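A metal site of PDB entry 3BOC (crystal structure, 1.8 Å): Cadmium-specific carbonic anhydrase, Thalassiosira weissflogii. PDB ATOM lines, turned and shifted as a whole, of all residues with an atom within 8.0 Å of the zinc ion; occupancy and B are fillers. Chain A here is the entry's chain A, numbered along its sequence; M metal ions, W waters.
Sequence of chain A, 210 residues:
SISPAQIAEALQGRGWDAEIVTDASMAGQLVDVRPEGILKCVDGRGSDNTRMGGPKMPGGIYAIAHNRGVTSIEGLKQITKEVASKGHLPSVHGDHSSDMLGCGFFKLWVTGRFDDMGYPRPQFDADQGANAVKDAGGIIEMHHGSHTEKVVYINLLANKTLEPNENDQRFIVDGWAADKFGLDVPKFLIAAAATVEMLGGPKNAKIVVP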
ATOM      1  N   LYS A  40      11.136  -6.451 -29.138  1.00  0.00           N
ATOM      2  CA  LYS A  40      11.979  -5.724 -28.186  1.00  0.00           C
ATOM      3  C   LYS A  40      11.723  -4.229 -28.155  1.00  0.00           C
ATOM      4  O   LYS A  40      10.850  -3.725 -28.862  1.00  0.00           O
ATOM      5  CB  LYS A  40      13.452  -5.983 -28.521  1.00  0.00           C
ATOM      6  CG  LYS A  40      13.759  -5.618 -29.971  1.00  0.00           C
ATOM      7  CD  LYS A  40      15.255  -5.556 -30.255  1.00  0.00           C
ATOM      8  CE  LYS A  40      15.812  -4.193 -29.930  1.00  0.00           C
ATOM      9  NZ  LYS A  40      17.303  -4.178 -29.964  1.00  0.00           N
ATOM     10  N   CYS A  41      12.520  -3.516 -27.371  1.00  0.00           N
ATOM     11  CA  CYS A  41      12.332  -2.073 -27.231  1.00  0.00           C
ATOM     12  C   CYS A  41      12.716  -1.169 -28.416  1.00  0.00           C
ATOM     13  O   CYS A  41      13.483  -1.570 -29.299  1.00  0.00           O
ATOM     14  CB  CYS A  41      13.060  -1.598 -25.964  1.00  0.00           C
ATOM     15  SG  CYS A  41      12.711   0.109 -25.451  1.00  0.00           S
ATOM     16  N   VAL A  42      12.161   0.053 -28.393  1.00  0.00           N
ATOM     17  CA  VAL A  42      12.361   1.079 -29.412  1.00  0.00           C
ATOM     18  C   VAL A  42      13.730   1.723 -29.312  1.00  0.00           C
ATOM     19  O   VAL A  42      14.135   2.493 -30.184  1.00  0.00           O
ATOM     20  CB  VAL A  42      11.303   2.192 -29.286  1.00  0.00           C
ATOM     21  CG1 VAL A  42       9.889   1.626 -29.474  1.00  0.00           C
ATOM     22  CG2 VAL A  42      11.390   2.833 -27.930  1.00  0.00           C
ATOM     23  N   ASP A  43      14.432   1.401 -28.219  1.00  0.00           N
ATOM     24  CA  ASP A  43      15.786   1.877 -27.889  1.00  0.00           C
ATOM     25  C   ASP A  43      16.683   1.865 -29.148  1.00  0.00           C
ATOM     26  O   ASP A  43      16.746   0.867 -29.868  1.00  0.00           O
ATOM     27  CB  ASP A  43      16.333   0.945 -26.807  1.00  0.00           C
ATOM     28  CG  ASP A  43      17.491   1.548 -26.033  1.00  0.00           C
ATOM     29  OD1 ASP A  43      18.433   2.024 -26.685  1.00  0.00           O
ATOM     30  OD2 ASP A  43      17.465   1.533 -24.779  1.00  0.00           O
ATOM     31  N   GLY A  44      17.402   2.944 -29.410  1.00  0.00           N
ATOM     32  CA  GLY A  44      18.254   2.964 -30.600  1.00  0.00           C
ATOM     33  C   GLY A  44      19.644   2.399 -30.435  1.00  0.00           C
ATOM     34  O   GLY A  44      20.409   2.313 -31.401  1.00  0.00           O
ATOM     35  N   ARG A  45      20.002   1.992 -29.221  1.00  0.00           N
ATOM     36  CA  ARG A  45      21.355   1.468 -28.980  1.00  0.00           C
ATOM     37  C   ARG A  45      21.626   0.040 -29.423  1.00  0.00           C
ATOM     38  O   ARG A  45      20.707  -0.749 -29.682  1.00  0.00           O
ATOM     39  CB  ARG A  45      21.689   1.568 -27.493  1.00  0.00           C
ATOM     40  CG  ARG A  45      21.789   2.983 -26.996  1.00  0.00           C
ATOM     41  CD  ARG A  45      21.914   3.002 -25.470  1.00  0.00           C
ATOM     42  NE  ARG A  45      20.723   2.464 -24.825  1.00  0.00           N
ATOM     43  CZ  ARG A  45      20.651   2.170 -23.519  1.00  0.00           C
ATOM     44  NH1 ARG A  45      21.713   2.360 -22.749  1.00  0.00           N
ATOM     45  NH2 ARG A  45      19.517   1.717 -22.992  1.00  0.00           N
ATOM     46  N   MET A  57       8.520  -2.147 -29.822  1.00  0.00           N
ATOM     47  CA  MET A  57       7.480  -1.487 -29.050  1.00  0.00           C
ATOM     48  C   MET A  57       8.153  -0.933 -27.776  1.00  0.00           C
ATOM     49  O   MET A  57       9.100  -1.524 -27.290  1.00  0.00           O
ATOM     50  CB  MET A  57       6.386  -2.483 -28.612  1.00  0.00           C
ATOM     51  CG  MET A  57       5.702  -3.262 -29.705  1.00  0.00           C
ATOM     52  SD  MET A  57       4.267  -4.136 -28.997  1.00  0.00           S
ATOM     53  CE  MET A  57       4.962  -4.772 -27.557  1.00  0.00           C
ATOM     54  N   PRO A  58       7.664   0.198 -27.236  1.00  0.00           N
ATOM     55  CA  PRO A  58       8.267   0.780 -26.027  1.00  0.00           C
ATOM     56  C   PRO A  58       8.402  -0.231 -24.889  1.00  0.00           C
ATOM     57  O   PRO A  58       7.410  -0.822 -24.474  1.00  0.00           O
ATOM     58  CB  PRO A  58       7.308   1.906 -25.682  1.00  0.00           C
ATOM     59  CG  PRO A  58       6.880   2.360 -27.028  1.00  0.00           C
ATOM     60  CD  PRO A  58       6.562   1.046 -27.703  1.00  0.00           C
ATOM     61  N   GLY A  59       9.615  -0.443 -24.376  1.00  0.00           N
ATOM     62  CA  GLY A  59       9.806  -1.402 -23.301  1.00  0.00           C
ATOM     63  C   GLY A  59       9.642  -2.874 -23.720  1.00  0.00           C
ATOM     64  O   GLY A  59       9.544  -3.768 -22.876  1.00  0.00           O
ATOM     65  N   GLY A  60       9.641  -3.144 -25.024  1.00  0.00           N
ATOM     66  CA  GLY A  60       9.472  -4.522 -25.428  1.00  0.00           C
ATOM     67  C   GLY A  60       8.025  -4.906 -25.109  1.00  0.00           C
ATOM     68  O   GLY A  60       7.097  -4.136 -25.431  1.00  0.00           O
ATOM     69  N   TYR A  62       6.504  -4.766 -22.426  1.00  0.00           N
ATOM     70  CA  TYR A  62       5.840  -3.896 -21.463  1.00  0.00           C
ATOM     71  C   TYR A  62       4.852  -2.947 -22.122  1.00  0.00           C
ATOM     72  O   TYR A  62       3.914  -2.488 -21.475  1.00  0.00           O
ATOM     73  CB  TYR A  62       6.856  -3.085 -20.667  1.00  0.00           C
ATOM     74  CG  TYR A  62       7.674  -3.850 -19.666  1.00  0.00           C
ATOM     75  CD1 TYR A  62       7.080  -4.770 -18.789  1.00  0.00           C
ATOM     76  CD2 TYR A  62       9.028  -3.601 -19.533  1.00  0.00           C
ATOM     77  CE1 TYR A  62       7.829  -5.397 -17.795  1.00  0.00           C
ATOM     78  CE2 TYR A  62       9.793  -4.214 -18.547  1.00  0.00           C
ATOM     79  CZ  TYR A  62       9.186  -5.107 -17.674  1.00  0.00           C
ATOM     80  OH  TYR A  62       9.938  -5.706 -16.703  1.00  0.00           O
ATOM     81  N   VAL A  92      12.205  -8.126 -22.758  1.00  0.00           N
ATOM     82  CA  VAL A  92      12.247  -6.844 -22.053  1.00  0.00           C
ATOM     83  C   VAL A  92      13.762  -6.660 -21.904  1.00  0.00           C
ATOM     84  O   VAL A  92      14.516  -7.600 -22.138  1.00  0.00           O
ATOM     85  CB  VAL A  92      11.521  -6.846 -20.669  1.00  0.00           C
ATOM     86  CG1 VAL A  92       9.994  -6.956 -20.912  1.00  0.00           C
ATOM     87  CG2 VAL A  92      12.026  -7.965 -19.784  1.00  0.00           C
ATOM     88  N   HIS A  93      14.238  -5.498 -21.485  1.00  0.00           N
ATOM     89  CA  HIS A  93      15.678  -5.312 -21.432  1.00  0.00           C
ATOM     90  C   HIS A  93      16.201  -4.374 -20.376  1.00  0.00           C
ATOM     91  O   HIS A  93      15.446  -3.675 -19.695  1.00  0.00           O
ATOM     92  CB  HIS A  93      16.172  -4.777 -22.795  1.00  0.00           C
ATOM     93  CG  HIS A  93      16.003  -3.290 -22.946  1.00  0.00           C
ATOM     94  ND1 HIS A  93      16.990  -2.381 -22.607  1.00  0.00           N
ATOM     95  CD2 HIS A  93      14.951  -2.541 -23.362  1.00  0.00           C
ATOM     96  CE1 HIS A  93      16.561  -1.147 -22.807  1.00  0.00           C
ATOM     97  NE2 HIS A  93      15.315  -1.219 -23.264  1.00  0.00           N
ATOM     98  N   GLY A  94      17.530  -4.371 -20.257  1.00  0.00           N
ATOM     99  CA  GLY A  94      18.216  -3.475 -19.344  1.00  0.00           C
ATOM    100  C   GLY A  94      19.439  -3.018 -20.108  1.00  0.00           C
ATOM    101  O   GLY A  94      19.437  -3.126 -21.317  1.00  0.00           O
ATOM    102  N   LEU A 101      17.268  -1.038 -14.891  1.00  0.00           N
ATOM    103  CA  LEU A 101      16.576   0.245 -15.021  1.00  0.00           C
ATOM    104  C   LEU A 101      17.097   0.907 -16.294  1.00  0.00           C
ATOM    105  O   LEU A 101      16.858   2.097 -16.539  1.00  0.00           O
ATOM    106  CB  LEU A 101      16.844   1.125 -13.799  1.00  0.00           C
ATOM    107  CG  LEU A 101      15.923   0.768 -12.615  1.00  0.00           C
ATOM    108  CD1 LEU A 101      16.427   1.450 -11.340  1.00  0.00           C
ATOM    109  CD2 LEU A 101      14.491   1.216 -12.906  1.00  0.00           C
ATOM    110  N   GLY A 102      17.819   0.136 -17.083  1.00  0.00           N
ATOM    111  CA  GLY A 102      18.381   0.619 -18.337  1.00  0.00           C
ATOM    112  C   GLY A 102      17.370   0.758 -19.454  1.00  0.00           C
ATOM    113  O   GLY A 102      17.738   1.119 -20.575  1.00  0.00           O
ATOM    114  N   CYS A 103      16.116   0.436 -19.189  1.00  0.00           N
ATOM    115  CA  CYS A 103      15.065   0.634 -20.204  1.00  0.00           C
ATOM    116  C   CYS A 103      14.305   1.912 -19.779  1.00  0.00           C
ATOM    117  O   CYS A 103      13.618   1.934 -18.743  1.00  0.00           O
ATOM    118  CB  CYS A 103      14.091  -0.533 -20.262  1.00  0.00           C
ATOM    119  SG  CYS A 103      12.671  -0.190 -21.386  1.00  0.00           S
ATOM    120  N   GLY A 104      14.455   2.968 -20.591  1.00  0.00           N
ATOM    121  CA  GLY A 104      13.824   4.248 -20.324  1.00  0.00           C
ATOM    122  C   GLY A 104      12.311   4.140 -20.145  1.00  0.00           C
ATOM    123  O   GLY A 104      11.755   4.735 -19.221  1.00  0.00           O
ATOM    124  N   PHE A 105      11.657   3.382 -21.016  1.00  0.00           N
ATOM    125  CA  PHE A 105      10.223   3.205 -20.902  1.00  0.00           C
ATOM    126  C   PHE A 105       9.836   2.587 -19.562  1.00  0.00           C
ATOM    127  O   PHE A 105       8.961   3.117 -18.868  1.00  0.00           O
ATOM    128  CB  PHE A 105       9.682   2.326 -22.027  1.00  0.00           C
ATOM    129  CG  PHE A 105       8.230   2.037 -21.906  1.00  0.00           C
ATOM    130  CD1 PHE A 105       7.283   2.978 -22.294  1.00  0.00           C
ATOM    131  CD2 PHE A 105       7.789   0.846 -21.340  1.00  0.00           C
ATOM    132  CE1 PHE A 105       5.920   2.742 -22.106  1.00  0.00           C
ATOM    133  CE2 PHE A 105       6.422   0.623 -21.150  1.00  0.00           C
ATOM    134  CZ  PHE A 105       5.499   1.565 -21.539  1.00  0.00           C
ATOM    135  N   PHE A 106      10.447   1.457 -19.172  1.00  0.00           N
ATOM    136  CA  PHE A 106      10.046   0.863 -17.904  1.00  0.00           C
ATOM    137  C   PHE A 106      10.352   1.786 -16.723  1.00  0.00           C
ATOM    138  O   PHE A 106       9.574   1.863 -15.773  1.00  0.00           O
ATOM    139  CB  PHE A 106      10.691  -0.504 -17.638  1.00  0.00           C
ATOM    140  CG  PHE A 106      10.155  -1.157 -16.402  1.00  0.00           C
ATOM    141  CD1 PHE A 106       8.875  -1.708 -16.400  1.00  0.00           C
ATOM    142  CD2 PHE A 106      10.851  -1.070 -15.207  1.00  0.00           C
ATOM    143  CE1 PHE A 106       8.295  -2.168 -15.226  1.00  0.00           C
ATOM    144  CE2 PHE A 106      10.260  -1.521 -14.016  1.00  0.00           C
ATOM    145  CZ  PHE A 106       8.997  -2.058 -14.022  1.00  0.00           C
ATOM    146  N   LYS A 107      11.484   2.471 -16.758  1.00  0.00           N
ATOM    147  CA  LYS A 107      11.857   3.389 -15.681  1.00  0.00           C
ATOM    148  C   LYS A 107      10.792   4.474 -15.541  1.00  0.00           C
ATOM    149  O   LYS A 107      10.350   4.780 -14.446  1.00  0.00           O
ATOM    150  CB  LYS A 107      13.229   4.012 -15.955  1.00  0.00           C
ATOM    151  CG  LYS A 107      13.688   5.040 -14.920  1.00  0.00           C
ATOM    152  CD  LYS A 107      15.162   5.355 -15.142  1.00  0.00           C
ATOM    153  CE  LYS A 107      15.582   6.677 -14.543  1.00  0.00           C
ATOM    154  NZ  LYS A 107      16.955   7.007 -15.016  1.00  0.00           N
ATOM    155  N   GLU A 141      17.147  -8.908 -22.897  1.00  0.00           N
ATOM    156  CA  GLU A 141      18.180  -8.256 -23.694  1.00  0.00           C
ATOM    157  C   GLU A 141      18.937  -7.240 -22.860  1.00  0.00           C
ATOM    158  O   GLU A 141      18.386  -6.704 -21.895  1.00  0.00           O
ATOM    159  CB  GLU A 141      17.514  -7.564 -24.900  1.00  0.00           C
ATOM    160  CG  GLU A 141      18.421  -6.661 -25.760  1.00  0.00           C
ATOM    161  CD  GLU A 141      17.658  -6.026 -26.905  1.00  0.00           C
ATOM    162  OE1 GLU A 141      16.478  -5.696 -26.699  1.00  0.00           O
ATOM    163  OE2 GLU A 141      18.214  -5.864 -28.016  1.00  0.00           O
ATOM    164  N   HIS A 143      21.401  -3.821 -23.464  1.00  0.00           N
ATOM    165  CA  HIS A 143      21.997  -2.837 -24.353  1.00  0.00           C
ATOM    166  C   HIS A 143      23.330  -2.310 -23.808  1.00  0.00           C
ATOM    167  O   HIS A 143      23.633  -2.434 -22.626  1.00  0.00           O
ATOM    168  CB  HIS A 143      21.050  -1.633 -24.531  1.00  0.00           C
ATOM    169  CG  HIS A 143      19.828  -1.941 -25.344  1.00  0.00           C
ATOM    170  ND1 HIS A 143      18.833  -2.792 -24.910  1.00  0.00           N
ATOM    171  CD2 HIS A 143      19.448  -1.530 -26.581  1.00  0.00           C
ATOM    172  CE1 HIS A 143      17.892  -2.886 -25.831  1.00  0.00           C
ATOM    173  NE2 HIS A 143      18.246  -2.126 -26.857  1.00  0.00           N
ATOM    174  N   HIS A 147      22.643   6.704 -25.454  1.00  0.00           N
ATOM    175  CA  HIS A 147      21.521   7.084 -26.316  1.00  0.00           C
ATOM    176  C   HIS A 147      21.912   8.296 -27.160  1.00  0.00           C
ATOM    177  O   HIS A 147      22.309   9.319 -26.611  1.00  0.00           O
ATOM    178  CB  HIS A 147      20.315   7.466 -25.463  1.00  0.00           C
ATOM    179  CG  HIS A 147      19.600   6.318 -24.820  1.00  0.00           C
ATOM    180  ND1 HIS A 147      18.781   5.473 -25.539  1.00  0.00           N
ATOM    181  CD2 HIS A 147      19.516   5.926 -23.533  1.00  0.00           C
ATOM    182  CE1 HIS A 147      18.207   4.612 -24.705  1.00  0.00           C
ATOM    183  NE2 HIS A 147      18.645   4.869 -23.484  1.00  0.00           N
ATOM    184  N   PHE A 171      14.955   5.860 -32.876  1.00  0.00           N
ATOM    185  CA  PHE A 171      13.964   5.133 -32.091  1.00  0.00           C
ATOM    186  C   PHE A 171      13.114   4.512 -33.184  1.00  0.00           C
ATOM    187  O   PHE A 171      12.842   5.178 -34.190  1.00  0.00           O
ATOM    188  CB  PHE A 171      13.084   6.094 -31.295  1.00  0.00           C
ATOM    189  CG  PHE A 171      13.702   6.553 -30.006  1.00  0.00           C
ATOM    190  CD1 PHE A 171      14.007   5.629 -29.011  1.00  0.00           C
ATOM    191  CD2 PHE A 171      13.979   7.889 -29.805  1.00  0.00           C
ATOM    192  CE1 PHE A 171      14.593   6.041 -27.807  1.00  0.00           C
ATOM    193  CE2 PHE A 171      14.551   8.315 -28.616  1.00  0.00           C
ATOM    194  CZ  PHE A 171      14.864   7.399 -27.615  1.00  0.00           C
ATOM    195  N   THR A 195       6.846   8.749 -24.287  1.00  0.00           N
ATOM    196  CA  THR A 195       8.076   8.115 -23.861  1.00  0.00           C
ATOM    197  C   THR A 195       9.261   8.869 -24.430  1.00  0.00           C
ATOM    198  O   THR A 195      10.178   9.246 -23.694  1.00  0.00           O
ATOM    199  CB  THR A 195       8.127   6.634 -24.314  1.00  0.00           C
ATOM    200  OG1 THR A 195       7.078   5.928 -23.657  1.00  0.00           O
ATOM    201  CG2 THR A 195       9.483   5.996 -23.976  1.00  0.00           C
ATOM    202  N   LEU A 199      11.957  11.123 -22.246  1.00  0.00           N
ATOM    203  CA  LEU A 199      13.350  10.699 -22.193  1.00  0.00           C
ATOM    204  C   LEU A 199      14.240  11.781 -22.793  1.00  0.00           C
ATOM    205  O   LEU A 199      15.453  11.605 -22.878  1.00  0.00           O
ATOM    206  CB  LEU A 199      13.587   9.387 -22.955  1.00  0.00           C
ATOM    207  CG  LEU A 199      12.942   8.151 -22.329  1.00  0.00           C
ATOM    208  CD1 LEU A 199      13.293   6.923 -23.148  1.00  0.00           C
ATOM    209  CD2 LEU A 199      13.404   7.999 -20.892  1.00  0.00           C
HETATM  210 ZN    ZN M   1      13.764   0.279 -23.414  1.00  0.00          ZN
HETATM  211  O   HOH W   1      12.600   3.339 -24.105  1.00  0.00           O
HETATM  212  O   HOH W   2      15.210   2.035 -23.500  1.00  0.00           O
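SG of Cys 41 sits close to N of Asp 43 (3.5 Å). The side-chain sulfur (SG) of Cys 41 lies close to the backbone NH (N) of Gly 59 (3.3 Å). The side-chain sulfur of Cys 103 lies close to the backbone NH of Phe 105, 3.7 Å away. ND1 of His 93 sits at hydrogen-bond distance from ND1 of His 143 (3.0 Å). N of Phe 106 lies close to SG of Cys 103.
N of Gly 104 touches the zinc ion (3.96 Å). Of the 27 residues printed, 4 come within 4 Å of the zinc ion. The nearest printed residue that does not touch the zinc ion is Asp 43 (4.1 Å).
The zinc ion is bound by NE2 of His 93 (2.2 Å), water W2 (2.3 Å), SG of Cys 41 (2.3 Å) and SG of Cys 103 (2.4 Å). The zinc ion has four donor atoms within binding distance.
Water W2 lies within hydrogen-bond range of the side-chain carboxylate (OD2) of Asp 43 (2.6 Å) and the backbone NH (N) of Gly 104 (3.1 Å).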
